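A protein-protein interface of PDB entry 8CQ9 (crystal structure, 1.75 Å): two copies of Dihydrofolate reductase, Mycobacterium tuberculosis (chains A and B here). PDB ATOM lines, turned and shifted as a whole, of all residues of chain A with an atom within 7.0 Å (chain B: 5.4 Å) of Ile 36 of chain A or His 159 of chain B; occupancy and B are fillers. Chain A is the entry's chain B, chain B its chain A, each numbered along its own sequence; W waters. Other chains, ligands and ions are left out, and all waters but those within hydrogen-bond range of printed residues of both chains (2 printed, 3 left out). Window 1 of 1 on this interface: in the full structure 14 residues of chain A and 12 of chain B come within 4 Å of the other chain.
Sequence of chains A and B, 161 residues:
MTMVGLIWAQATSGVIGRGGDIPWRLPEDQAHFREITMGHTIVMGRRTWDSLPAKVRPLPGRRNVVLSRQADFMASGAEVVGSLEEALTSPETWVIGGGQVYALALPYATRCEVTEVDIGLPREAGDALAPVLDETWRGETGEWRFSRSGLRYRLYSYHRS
Hydrophobic or aromatic side chains of chain A that line the printed part of chain B: Ala 31 and Met 38.
Printed residues of chain B that touch a printed residue of chain A: Arg 111, Arg 138, His 159, Arg 160 and Ser 161.
Arg 111 of chain B touches its own counterpart, Arg 111 of chain A.
Among the printed residues, pairs that only touch across the chains: Ala 31 of chain A with Arg 138 of chain B (3.8 Å), Glu 35 of chain A with Arg 138 of chain B (3.98 Å), Glu 35 of chain A with Arg 160 of chain B (3.5 Å), Ile 36 of chain A with His 159 of chain B (3.7 Å) and Met 38 of chain A with Ser 161 of chain B (3.5 Å).
A ring nitrogen (NE2) of His 159 of chain B is in hydrogen-bond range of the backbone carbonyl oxygen (O) of Glu 35 of chain A.
The backbone carbonyl oxygen (O) of Glu 35 of chain A is in hydrogen-bond range of the side-chain hydroxyl (OG) of Ser 161 of chain B, 2.8 Å away.
The guanidinium group (NH1) of Arg 111 of chain B sits close to the guanidinium group (NH1) of Arg 111 of chain A (3.3 Å).
O of Thr 110 of chain B sits at hydrogen-bond distance from ND1 of His 159 of chain B (3.2 Å).
O of Thr 110 of chain B sits at hydrogen-bond distance from N of Arg 160 of chain B (3.1 Å).
NH1 of Arg 160 of chain B is in hydrogen-bond range of OG1 of Thr 136 of chain B (3.2 Å).
N of Arg 138 of chain B sits at hydrogen-bond distance from O of His 159 of chain B (2.6 Å).
The backbone NH of Leu 6 of chain A sits at hydrogen-bond distance from the backbone carbonyl oxygen of Arg 111 of chain A (2.9 Å).
The side-chain carboxylate (OE2) of Glu 113 of chain A lies within salt-bridge range of the guanidinium group (NH2) of Arg 111 of chain A (2.9 Å).
Of chain A, only Glu 35 and Ile 36 come within 4 Å of His 159 of chain B.
Of the printed residues of chain A, Arg 160 of chain B touches Glu 35.
Of the printed residues of chain B, Ala 31 of chain A touches Arg 138 (3.8 Å).
Thr 136 of chain B touches none of the printed residues of chain A.
Gln 30 of chain A touches none of the printed residues of chain B.
The nearest residue of chain A that does not touch His 159 of chain B is Arg 111 of chain A (5.6 Å).
Water W2 bridges NH1 of Arg 111 of chain B and NH1 of Arg 111 of chain A.
Water W1 lies within hydrogen-bond range of the backbone carbonyl oxygen (O) of Thr 136 of chain B and the side-chain carboxylate (OE2) of Glu 35 of chain A.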
ATOM      1  N   MET A   3      16.817  23.892  10.580  1.00  0.00           N
ATOM      2  CA  MET A   3      15.886  23.324  11.551  1.00  0.00           C
ATOM      3  C   MET A   3      15.220  22.125  10.899  1.00  0.00           C
ATOM      4  O   MET A   3      14.600  22.255   9.834  1.00  0.00           O
ATOM      5  CB  MET A   3      14.812  24.330  11.965  1.00  0.00           C
ATOM      6  CG  MET A   3      13.924  23.882  13.139  1.00  0.00           C
ATOM      7  SD  MET A   3      12.672  22.559  12.990  1.00  0.00           S
ATOM      8  CE  MET A   3      11.763  22.980  11.493  1.00  0.00           C
ATOM      9  N   LEU A   6       9.984  16.856  12.541  1.00  0.00           N
ATOM     10  CA  LEU A   6       9.155  15.725  12.134  1.00  0.00           C
ATOM     11  C   LEU A   6       7.702  16.101  12.352  1.00  0.00           C
ATOM     12  O   LEU A   6       7.369  16.703  13.369  1.00  0.00           O
ATOM     13  CB  LEU A   6       9.470  14.463  12.958  1.00  0.00           C
ATOM     14  CG  LEU A   6      10.577  13.590  12.381  1.00  0.00           C
ATOM     15  CD1 LEU A   6      11.858  14.392  12.248  1.00  0.00           C
ATOM     16  CD2 LEU A   6      10.810  12.338  13.235  1.00  0.00           C
ATOM     17  N   ILE A   7       6.829  15.751  11.416  1.00  0.00           N
ATOM     18  CA  ILE A   7       5.399  15.964  11.606  1.00  0.00           C
ATOM     19  C   ILE A   7       4.647  14.689  11.222  1.00  0.00           C
ATOM     20  O   ILE A   7       4.890  14.110  10.155  1.00  0.00           O
ATOM     21  CB  ILE A   7       4.912  17.193  10.804  1.00  0.00           C
ATOM     22  CG1 ILE A   7       3.435  17.483  11.081  1.00  0.00           C
ATOM     23  CG2 ILE A   7       5.256  17.056   9.292  1.00  0.00           C
ATOM     24  CD1 ILE A   7       2.961  18.806  10.461  1.00  0.00           C
ATOM     25  N   GLN A  30      -5.112  17.948   8.399  1.00  0.00           N
ATOM     26  CA  GLN A  30      -4.561  18.226   7.076  1.00  0.00           C
ATOM     27  C   GLN A  30      -4.298  19.716   6.898  1.00  0.00           C
ATOM     28  O   GLN A  30      -3.260  20.118   6.358  1.00  0.00           O
ATOM     29  CB  GLN A  30      -5.493  17.703   5.984  1.00  0.00           C
ATOM     30  CG  GLN A  30      -4.993  18.036   4.584  1.00  0.00           C
ATOM     31  CD  GLN A  30      -5.933  17.581   3.504  1.00  0.00           C
ATOM     32  OE1 GLN A  30      -6.859  16.812   3.759  1.00  0.00           O
ATOM     33  NE2 GLN A  30      -5.731  18.089   2.288  1.00  0.00           N
ATOM     34  N   ALA A  31      -5.215  20.560   7.362  1.00  0.00           N
ATOM     35  CA  ALA A  31      -4.968  21.994   7.256  1.00  0.00           C
ATOM     36  C   ALA A  31      -3.778  22.403   8.118  1.00  0.00           C
ATOM     37  O   ALA A  31      -2.990  23.276   7.734  1.00  0.00           O
ATOM     38  CB  ALA A  31      -6.226  22.771   7.638  1.00  0.00           C
ATOM     39  N   HIS A  32      -3.621  21.765   9.280  1.00  0.00           N
ATOM     40  CA  HIS A  32      -2.473  22.026  10.145  1.00  0.00           C
ATOM     41  C   HIS A  32      -1.166  21.587   9.478  1.00  0.00           C
ATOM     42  O   HIS A  32      -0.165  22.319   9.488  1.00  0.00           O
ATOM     43  CB  HIS A  32      -2.680  21.290  11.477  1.00  0.00           C
ATOM     44  CG  HIS A  32      -1.580  21.498  12.468  1.00  0.00           C
ATOM     45  ND1 HIS A  32      -0.811  20.465  12.955  1.00  0.00           N
ATOM     46  CD2 HIS A  32      -1.132  22.622  13.072  1.00  0.00           C
ATOM     47  CE1 HIS A  32       0.058  20.942  13.829  1.00  0.00           C
ATOM     48  NE2 HIS A  32      -0.109  22.251  13.909  1.00  0.00           N
ATOM     49  N   PHE A  33      -1.154  20.377   8.916  1.00  0.00           N
ATOM     50  CA  PHE A  33       0.010  19.886   8.184  1.00  0.00           C
ATOM     51  C   PHE A  33       0.378  20.826   7.039  1.00  0.00           C
ATOM     52  O   PHE A  33       1.559  21.132   6.818  1.00  0.00           O
ATOM     53  CB  PHE A  33      -0.307  18.487   7.653  1.00  0.00           C
ATOM     54  CG  PHE A  33       0.655  17.987   6.617  1.00  0.00           C
ATOM     55  CD1 PHE A  33       1.823  17.328   6.994  1.00  0.00           C
ATOM     56  CD2 PHE A  33       0.384  18.148   5.269  1.00  0.00           C
ATOM     57  CE1 PHE A  33       2.711  16.844   6.051  1.00  0.00           C
ATOM     58  CE2 PHE A  33       1.278  17.660   4.302  1.00  0.00           C
ATOM     59  CZ  PHE A  33       2.443  17.026   4.692  1.00  0.00           C
ATOM     60  N   ARG A  34      -0.627  21.298   6.309  1.00  0.00           N
ATOM     61  CA  ARG A  34      -0.378  22.230   5.211  1.00  0.00           C
ATOM     62  C   ARG A  34       0.285  23.507   5.711  1.00  0.00           C
ATOM     63  O   ARG A  34       1.268  23.980   5.128  1.00  0.00           O
ATOM     64  CB  ARG A  34      -1.689  22.561   4.520  1.00  0.00           C
ATOM     65  CG  ARG A  34      -1.543  23.527   3.380  1.00  0.00           C
ATOM     66  CD  ARG A  34      -2.842  23.584   2.600  1.00  0.00           C
ATOM     67  NE  ARG A  34      -2.794  24.629   1.584  1.00  0.00           N
ATOM     68  CZ  ARG A  34      -3.156  25.889   1.786  1.00  0.00           C
ATOM     69  NH1 ARG A  34      -3.579  26.275   2.983  1.00  0.00           N
ATOM     70  NH2 ARG A  34      -3.080  26.765   0.791  1.00  0.00           N
ATOM     71  N   GLU A  35      -0.250  24.088   6.794  1.00  0.00           N
ATOM     72  CA  GLU A  35       0.292  25.340   7.325  1.00  0.00           C
ATOM     73  C   GLU A  35       1.739  25.185   7.775  1.00  0.00           C
ATOM     74  O   GLU A  35       2.580  26.053   7.493  1.00  0.00           O
ATOM     75  CB  GLU A  35      -0.567  25.844   8.486  1.00  0.00           C
ATOM     76  CG  GLU A  35      -0.440  27.353   8.786  1.00  0.00           C
ATOM     77  CD  GLU A  35      -1.193  28.221   7.786  1.00  0.00           C
ATOM     78  OE1 GLU A  35      -2.049  27.666   7.070  1.00  0.00           O
ATOM     79  OE2 GLU A  35      -0.928  29.448   7.703  1.00  0.00           O
ATOM     80  N   ILE A  36       2.053  24.084   8.466  1.00  0.00           N
ATOM     81  CA  ILE A  36       3.402  23.928   9.000  1.00  0.00           C
ATOM     82  C   ILE A  36       4.410  23.668   7.898  1.00  0.00           C
ATOM     83  O   ILE A  36       5.554  24.124   7.986  1.00  0.00           O
ATOM     84  CB  ILE A  36       3.460  22.815  10.062  1.00  0.00           C
ATOM     85  CG1 ILE A  36       2.609  23.177  11.266  1.00  0.00           C
ATOM     86  CG2 ILE A  36       4.875  22.552  10.507  1.00  0.00           C
ATOM     87  CD1 ILE A  36       2.508  22.099  12.220  1.00  0.00           C
ATOM     88  N   THR A  37       4.022  22.934   6.852  1.00  0.00           N
ATOM     89  CA  THR A  37       5.005  22.543   5.849  1.00  0.00           C
ATOM     90  C   THR A  37       5.122  23.518   4.680  1.00  0.00           C
ATOM     91  O   THR A  37       6.185  23.562   4.054  1.00  0.00           O
ATOM     92  CB  THR A  37       4.702  21.138   5.306  1.00  0.00           C
ATOM     93  OG1 THR A  37       3.380  21.082   4.747  1.00  0.00           O
ATOM     94  CG2 THR A  37       4.857  20.077   6.438  1.00  0.00           C
ATOM     95  N   MET A  38       4.066  24.255   4.354  1.00  0.00           N
ATOM     96  CA  MET A  38       4.080  25.206   3.237  1.00  0.00           C
ATOM     97  C   MET A  38       5.330  26.059   3.183  1.00  0.00           C
ATOM     98  O   MET A  38       5.734  26.653   4.184  1.00  0.00           O
ATOM     99  CB  MET A  38       2.855  26.115   3.298  1.00  0.00           C
ATOM    100  CG  MET A  38       2.634  26.921   2.028  1.00  0.00           C
ATOM    101  SD  MET A  38       2.501  25.919   0.563  1.00  0.00           S
ATOM    102  CE  MET A  38       0.900  25.159   0.819  1.00  0.00           C
ATOM    103  N   GLY A  39       5.881  26.194   1.977  1.00  0.00           N
ATOM    104  CA  GLY A  39       7.054  27.006   1.739  1.00  0.00           C
ATOM    105  C   GLY A  39       8.377  26.307   1.979  1.00  0.00           C
ATOM    106  O   GLY A  39       9.414  26.778   1.499  1.00  0.00           O
ATOM    107  N   HIS A  40       8.368  25.178   2.656  1.00  0.00           N
ATOM    108  CA  HIS A  40       9.588  24.564   3.134  1.00  0.00           C
ATOM    109  C   HIS A  40       9.911  23.310   2.336  1.00  0.00           C
ATOM    110  O   HIS A  40       9.159  22.881   1.451  1.00  0.00           O
ATOM    111  CB  HIS A  40       9.447  24.249   4.630  1.00  0.00           C
ATOM    112  CG  HIS A  40       9.076  25.449   5.449  1.00  0.00           C
ATOM    113  ND1 HIS A  40       9.772  26.638   5.375  1.00  0.00           N
ATOM    114  CD2 HIS A  40       8.064  25.659   6.321  1.00  0.00           C
ATOM    115  CE1 HIS A  40       9.222  27.521   6.197  1.00  0.00           C
ATOM    116  NE2 HIS A  40       8.183  26.954   6.776  1.00  0.00           N
ATOM    117  N   ARG A  62       5.996  23.435  -1.970  1.00  0.00           N
ATOM    118  CA  ARG A  62       7.012  22.869  -1.102  1.00  0.00           C
ATOM    119  C   ARG A  62       8.045  22.197  -1.990  1.00  0.00           C
ATOM    120  O   ARG A  62       7.723  21.723  -3.078  1.00  0.00           O
ATOM    121  CB  ARG A  62       6.380  21.879  -0.096  1.00  0.00           C
ATOM    122  CG  ARG A  62       5.696  22.618   1.048  1.00  0.00           C
ATOM    123  CD  ARG A  62       4.480  21.870   1.597  1.00  0.00           C
ATOM    124  NE  ARG A  62       3.355  21.881   0.669  1.00  0.00           N
ATOM    125  CZ  ARG A  62       2.149  21.427   0.977  1.00  0.00           C
ATOM    126  NH1 ARG A  62       1.932  20.918   2.198  1.00  0.00           N
ATOM    127  NH2 ARG A  62       1.176  21.457   0.067  1.00  0.00           N
ATOM    128  N   GLU A  92      14.643  25.318   6.770  1.00  0.00           N
ATOM    129  CA  GLU A  92      13.587  24.594   7.462  1.00  0.00           C
ATOM    130  C   GLU A  92      13.209  23.394   6.611  1.00  0.00           C
ATOM    131  O   GLU A  92      12.831  23.554   5.449  1.00  0.00           O
ATOM    132  CB  GLU A  92      12.375  25.490   7.693  1.00  0.00           C
ATOM    133  CG  GLU A  92      11.250  24.841   8.503  1.00  0.00           C
ATOM    134  CD  GLU A  92      10.291  25.857   9.101  1.00  0.00           C
ATOM    135  OE1 GLU A  92       9.245  25.438   9.647  1.00  0.00           O
ATOM    136  OE2 GLU A  92      10.559  27.074   8.987  1.00  0.00           O
ATOM    137  N   TRP A  94      10.877  19.728   6.832  1.00  0.00           N
ATOM    138  CA  TRP A  94       9.911  18.924   7.564  1.00  0.00           C
ATOM    139  C   TRP A  94       9.944  17.515   7.004  1.00  0.00           C
ATOM    140  O   TRP A  94       9.776  17.330   5.794  1.00  0.00           O
ATOM    141  CB  TRP A  94       8.513  19.526   7.465  1.00  0.00           C
ATOM    142  CG  TRP A  94       8.444  20.688   8.371  1.00  0.00           C
ATOM    143  CD1 TRP A  94       8.650  22.002   8.042  1.00  0.00           C
ATOM    144  CD2 TRP A  94       8.264  20.647   9.785  1.00  0.00           C
ATOM    145  NE1 TRP A  94       8.576  22.787   9.174  1.00  0.00           N
ATOM    146  CE2 TRP A  94       8.326  21.982  10.253  1.00  0.00           C
ATOM    147  CE3 TRP A  94       8.009  19.621  10.702  1.00  0.00           C
ATOM    148  CZ2 TRP A  94       8.166  22.309  11.597  1.00  0.00           C
ATOM    149  CZ3 TRP A  94       7.856  19.948  12.041  1.00  0.00           C
ATOM    150  CH2 TRP A  94       7.931  21.291  12.470  1.00  0.00           C
ATOM    151  N   ARG A 111      12.344  19.476  16.502  1.00  0.00           N
ATOM    152  CA  ARG A 111      10.921  19.550  16.808  1.00  0.00           C
ATOM    153  C   ARG A 111      10.197  18.344  16.220  1.00  0.00           C
ATOM    154  O   ARG A 111      10.576  17.840  15.161  1.00  0.00           O
ATOM    155  CB  ARG A 111      10.308  20.831  16.235  1.00  0.00           C
ATOM    156  CG  ARG A 111      10.930  22.102  16.780  1.00  0.00           C
ATOM    157  CD  ARG A 111      10.401  23.326  16.016  1.00  0.00           C
ATOM    158  NE  ARG A 111       8.949  23.324  15.952  1.00  0.00           N
ATOM    159  CZ  ARG A 111       8.236  24.088  15.132  1.00  0.00           C
ATOM    160  NH1 ARG A 111       8.846  24.918  14.293  1.00  0.00           N
ATOM    161  NH2 ARG A 111       6.911  24.024  15.146  1.00  0.00           N
ATOM    162  N   GLU A 113       5.972  17.810  15.537  1.00  0.00           N
ATOM    163  CA  GLU A 113       4.590  18.264  15.620  1.00  0.00           C
ATOM    164  C   GLU A 113       3.702  17.039  15.444  1.00  0.00           C
ATOM    165  O   GLU A 113       3.648  16.451  14.357  1.00  0.00           O
ATOM    166  CB  GLU A 113       4.295  19.320  14.561  1.00  0.00           C
ATOM    167  CG  GLU A 113       5.006  20.626  14.812  1.00  0.00           C
ATOM    168  CD  GLU A 113       4.526  21.331  16.081  1.00  0.00           C
ATOM    169  OE1 GLU A 113       3.361  21.150  16.473  1.00  0.00           O
ATOM    170  OE2 GLU A 113       5.318  22.085  16.689  1.00  0.00           O
ATOM    171  N   VAL A 114       3.027  16.649  16.518  1.00  0.00           N
ATOM    172  CA  VAL A 114       2.331  15.371  16.595  1.00  0.00           C
ATOM    173  C   VAL A 114       0.848  15.639  16.753  1.00  0.00           C
ATOM    174  O   VAL A 114       0.438  16.367  17.661  1.00  0.00           O
ATOM    175  CB  VAL A 114       2.852  14.526  17.767  1.00  0.00           C
ATOM    176  CG1 VAL A 114       2.142  13.160  17.798  1.00  0.00           C
ATOM    177  CG2 VAL A 114       4.387  14.383  17.688  1.00  0.00           C
ATOM    178  N   LEU A 155      -3.160  18.038  19.700  1.00  0.00           N
ATOM    179  CA  LEU A 155      -1.865  18.378  19.131  1.00  0.00           C
ATOM    180  C   LEU A 155      -0.797  18.407  20.216  1.00  0.00           C
ATOM    181  O   LEU A 155      -1.043  18.887  21.326  1.00  0.00           O
ATOM    182  CB  LEU A 155      -1.927  19.744  18.449  1.00  0.00           C
ATOM    183  CG  LEU A 155      -2.821  19.893  17.220  1.00  0.00           C
ATOM    184  CD1 LEU A 155      -2.498  21.209  16.504  1.00  0.00           C
ATOM    185  CD2 LEU A 155      -2.710  18.704  16.270  1.00  0.00           C
ATOM    186  N   SER A 157       3.250  19.796  20.549  1.00  0.00           N
ATOM    187  CA  SER A 157       4.395  20.483  19.955  1.00  0.00           C
ATOM    188  C   SER A 157       5.631  20.133  20.781  1.00  0.00           C
ATOM    189  O   SER A 157       5.889  20.749  21.819  1.00  0.00           O
ATOM    190  CB  SER A 157       4.167  21.996  19.889  1.00  0.00           C
ATOM    191  OG  SER A 157       3.141  22.341  18.976  1.00  0.00           O
ATOM    192  N   THR B 110       6.591  33.828  11.737  1.00  0.00           N
ATOM    193  CA  THR B 110       5.666  32.727  11.485  1.00  0.00           C
ATOM    194  C   THR B 110       5.239  31.998  12.753  1.00  0.00           C
ATOM    195  O   THR B 110       4.380  31.117  12.689  1.00  0.00           O
ATOM    196  CB  THR B 110       6.279  31.708  10.513  1.00  0.00           C
ATOM    197  OG1 THR B 110       7.628  31.445  10.905  1.00  0.00           O
ATOM    198  CG2 THR B 110       6.257  32.267   9.118  1.00  0.00           C
ATOM    199  N   ARG B 111       5.817  32.325  13.900  1.00  0.00           N
ATOM    200  CA  ARG B 111       5.355  31.774  15.156  1.00  0.00           C
ATOM    201  C   ARG B 111       5.273  32.889  16.183  1.00  0.00           C
ATOM    202  O   ARG B 111       6.124  33.778  16.203  1.00  0.00           O
ATOM    203  CB  ARG B 111       6.302  30.688  15.671  1.00  0.00           C
ATOM    204  CG  ARG B 111       6.396  29.472  14.762  1.00  0.00           C
ATOM    205  CD  ARG B 111       7.459  28.532  15.316  1.00  0.00           C
ATOM    206  NE  ARG B 111       7.086  27.999  16.624  1.00  0.00           N
ATOM    207  CZ  ARG B 111       7.878  27.224  17.357  1.00  0.00           C
ATOM    208  NH1 ARG B 111       9.093  26.937  16.914  1.00  0.00           N
ATOM    209  NH2 ARG B 111       7.464  26.737  18.527  1.00  0.00           N
ATOM    210  N   CYS B 112       4.242  32.839  17.017  1.00  0.00           N
ATOM    211  CA  CYS B 112       4.171  33.630  18.237  1.00  0.00           C
ATOM    212  C   CYS B 112       3.859  32.671  19.370  1.00  0.00           C
ATOM    213  O   CYS B 112       2.816  32.015  19.352  1.00  0.00           O
ATOM    214  CB  CYS B 112       3.088  34.705  18.166  1.00  0.00           C
ATOM    215  SG  CYS B 112       3.386  35.983  16.935  1.00  0.00           S
ATOM    216  N   THR B 136      -4.388  36.004   9.511  1.00  0.00           N
ATOM    217  CA  THR B 136      -3.467  35.011   8.978  1.00  0.00           C
ATOM    218  C   THR B 136      -2.911  34.076  10.052  1.00  0.00           C
ATOM    219  O   THR B 136      -2.360  33.021   9.712  1.00  0.00           O
ATOM    220  CB  THR B 136      -2.330  35.723   8.236  1.00  0.00           C
ATOM    221  OG1 THR B 136      -1.556  36.504   9.155  1.00  0.00           O
ATOM    222  CG2 THR B 136      -2.897  36.652   7.176  1.00  0.00           C
ATOM    223  N   TRP B 137      -3.090  34.397  11.336  1.00  0.00           N
ATOM    224  CA  TRP B 137      -2.480  33.624  12.415  1.00  0.00           C
ATOM    225  C   TRP B 137      -3.390  32.497  12.892  1.00  0.00           C
ATOM    226  O   TRP B 137      -4.554  32.727  13.230  1.00  0.00           O
ATOM    227  CB  TRP B 137      -2.129  34.542  13.581  1.00  0.00           C
ATOM    228  CG  TRP B 137      -0.981  35.402  13.261  1.00  0.00           C
ATOM    229  CD1 TRP B 137      -1.025  36.680  12.821  1.00  0.00           C
ATOM    230  CD2 TRP B 137       0.402  35.048  13.343  1.00  0.00           C
ATOM    231  NE1 TRP B 137       0.243  37.159  12.618  1.00  0.00           N
ATOM    232  CE2 TRP B 137       1.141  36.175  12.940  1.00  0.00           C
ATOM    233  CE3 TRP B 137       1.089  33.892  13.727  1.00  0.00           C
ATOM    234  CZ2 TRP B 137       2.524  36.180  12.905  1.00  0.00           C
ATOM    235  CZ3 TRP B 137       2.454  33.894  13.681  1.00  0.00           C
ATOM    236  CH2 TRP B 137       3.163  35.030  13.270  1.00  0.00           C
ATOM    237  N   ARG B 138      -2.837  31.289  12.945  1.00  0.00           N
ATOM    238  CA  ARG B 138      -3.545  30.101  13.396  1.00  0.00           C
ATOM    239  C   ARG B 138      -3.119  29.797  14.824  1.00  0.00           C
ATOM    240  O   ARG B 138      -1.922  29.670  15.106  1.00  0.00           O
ATOM    241  CB  ARG B 138      -3.236  28.918  12.474  1.00  0.00           C
ATOM    242  CG  ARG B 138      -3.437  27.534  13.077  1.00  0.00           C
ATOM    243  CD  ARG B 138      -3.029  26.432  12.088  1.00  0.00           C
ATOM    244  NE  ARG B 138      -3.760  26.541  10.829  1.00  0.00           N
ATOM    245  CZ  ARG B 138      -4.881  25.880  10.558  1.00  0.00           C
ATOM    246  NH1 ARG B 138      -5.494  26.055   9.390  1.00  0.00           N
ATOM    247  NH2 ARG B 138      -5.393  25.044  11.450  1.00  0.00           N
ATOM    248  N   GLY B 139      -4.091  29.660  15.719  1.00  0.00           N
ATOM    249  CA  GLY B 139      -3.764  29.604  17.129  1.00  0.00           C
ATOM    250  C   GLY B 139      -4.435  28.515  17.937  1.00  0.00           C
ATOM    251  O   GLY B 139      -5.662  28.461  18.047  1.00  0.00           O
ATOM    252  N   SER B 157       0.180  28.831  21.076  1.00  0.00           N
ATOM    253  CA  SER B 157       1.216  28.679  20.055  1.00  0.00           C
ATOM    254  C   SER B 157       0.588  29.090  18.731  1.00  0.00           C
ATOM    255  O   SER B 157      -0.009  28.274  18.026  1.00  0.00           O
ATOM    256  CB  SER B 157       1.752  27.253  20.003  1.00  0.00           C
ATOM    257  OG  SER B 157       2.309  26.875  21.247  1.00  0.00           O
ATOM    258  N   TYR B 158       0.711  30.370  18.407  1.00  0.00           N
ATOM    259  CA  TYR B 158       0.204  30.874  17.143  1.00  0.00           C
ATOM    260  C   TYR B 158       1.180  30.541  16.034  1.00  0.00           C
ATOM    261  O   TYR B 158       2.392  30.472  16.243  1.00  0.00           O
ATOM    262  CB  TYR B 158      -0.001  32.387  17.177  1.00  0.00           C
ATOM    263  CG  TYR B 158      -1.163  32.862  18.013  1.00  0.00           C
ATOM    264  CD1 TYR B 158      -0.963  33.330  19.312  1.00  0.00           C
ATOM    265  CD2 TYR B 158      -2.455  32.888  17.503  1.00  0.00           C
ATOM    266  CE1 TYR B 158      -2.010  33.778  20.074  1.00  0.00           C
ATOM    267  CE2 TYR B 158      -3.515  33.343  18.272  1.00  0.00           C
ATOM    268  CZ  TYR B 158      -3.285  33.781  19.559  1.00  0.00           C
ATOM    269  OH  TYR B 158      -4.329  34.242  20.345  1.00  0.00           O
ATOM    270  N   HIS B 159       0.643  30.384  14.836  1.00  0.00           N
ATOM    271  CA  HIS B 159       1.468  29.975  13.724  1.00  0.00           C
ATOM    272  C   HIS B 159       0.791  30.389  12.431  1.00  0.00           C
ATOM    273  O   HIS B 159      -0.438  30.466  12.347  1.00  0.00           O
ATOM    274  CB  HIS B 159       1.687  28.463  13.739  1.00  0.00           C
ATOM    275  CG  HIS B 159       2.444  27.961  12.556  1.00  0.00           C
ATOM    276  ND1 HIS B 159       3.821  27.941  12.515  1.00  0.00           N
ATOM    277  CD2 HIS B 159       2.020  27.523  11.345  1.00  0.00           C
ATOM    278  CE1 HIS B 159       4.214  27.461  11.349  1.00  0.00           C
ATOM    279  NE2 HIS B 159       3.142  27.211  10.615  1.00  0.00           N
ATOM    280  N   ARG B 160       1.621  30.635  11.419  1.00  0.00           N
ATOM    281  CA  ARG B 160       1.161  30.858  10.061  1.00  0.00           C
ATOM    282  C   ARG B 160       2.280  30.466   9.110  1.00  0.00           C
ATOM    283  O   ARG B 160       3.455  30.478   9.478  1.00  0.00           O
ATOM    284  CB  ARG B 160       0.761  32.317   9.836  1.00  0.00           C
ATOM    285  CG  ARG B 160       1.944  33.282   9.831  1.00  0.00           C
ATOM    286  CD  ARG B 160       1.494  34.703   9.488  1.00  0.00           C
ATOM    287  NE  ARG B 160       2.596  35.662   9.640  1.00  0.00           N
ATOM    288  CZ  ARG B 160       2.546  36.945   9.300  1.00  0.00           C
ATOM    289  NH1 ARG B 160       1.438  37.475   8.776  1.00  0.00           N
ATOM    290  NH2 ARG B 160       3.615  37.706   9.485  1.00  0.00           N
ATOM    291  N   SER B 161       1.906  30.131   7.878  1.00  0.00           N
ATOM    292  CA  SER B 161       2.908  29.897   6.849  1.00  0.00           C
ATOM    293  C   SER B 161       3.614  31.203   6.546  1.00  0.00           C
ATOM    294  O   SER B 161       4.827  31.239   6.308  1.00  0.00           O
ATOM    295  CB  SER B 161       2.265  29.331   5.579  1.00  0.00           C
ATOM    296  OG  SER B 161       1.589  28.133   5.876  1.00  0.00           O
ATOM    297  OXT SER B 161       2.964  32.252   6.542  1.00  0.00           O
HETATM  298  O   HOH W   1      -1.908  32.051   7.268  1.00  0.00           O
HETATM  299  O   HOH W   2      11.036  27.000  15.272  1.00  0.00           O
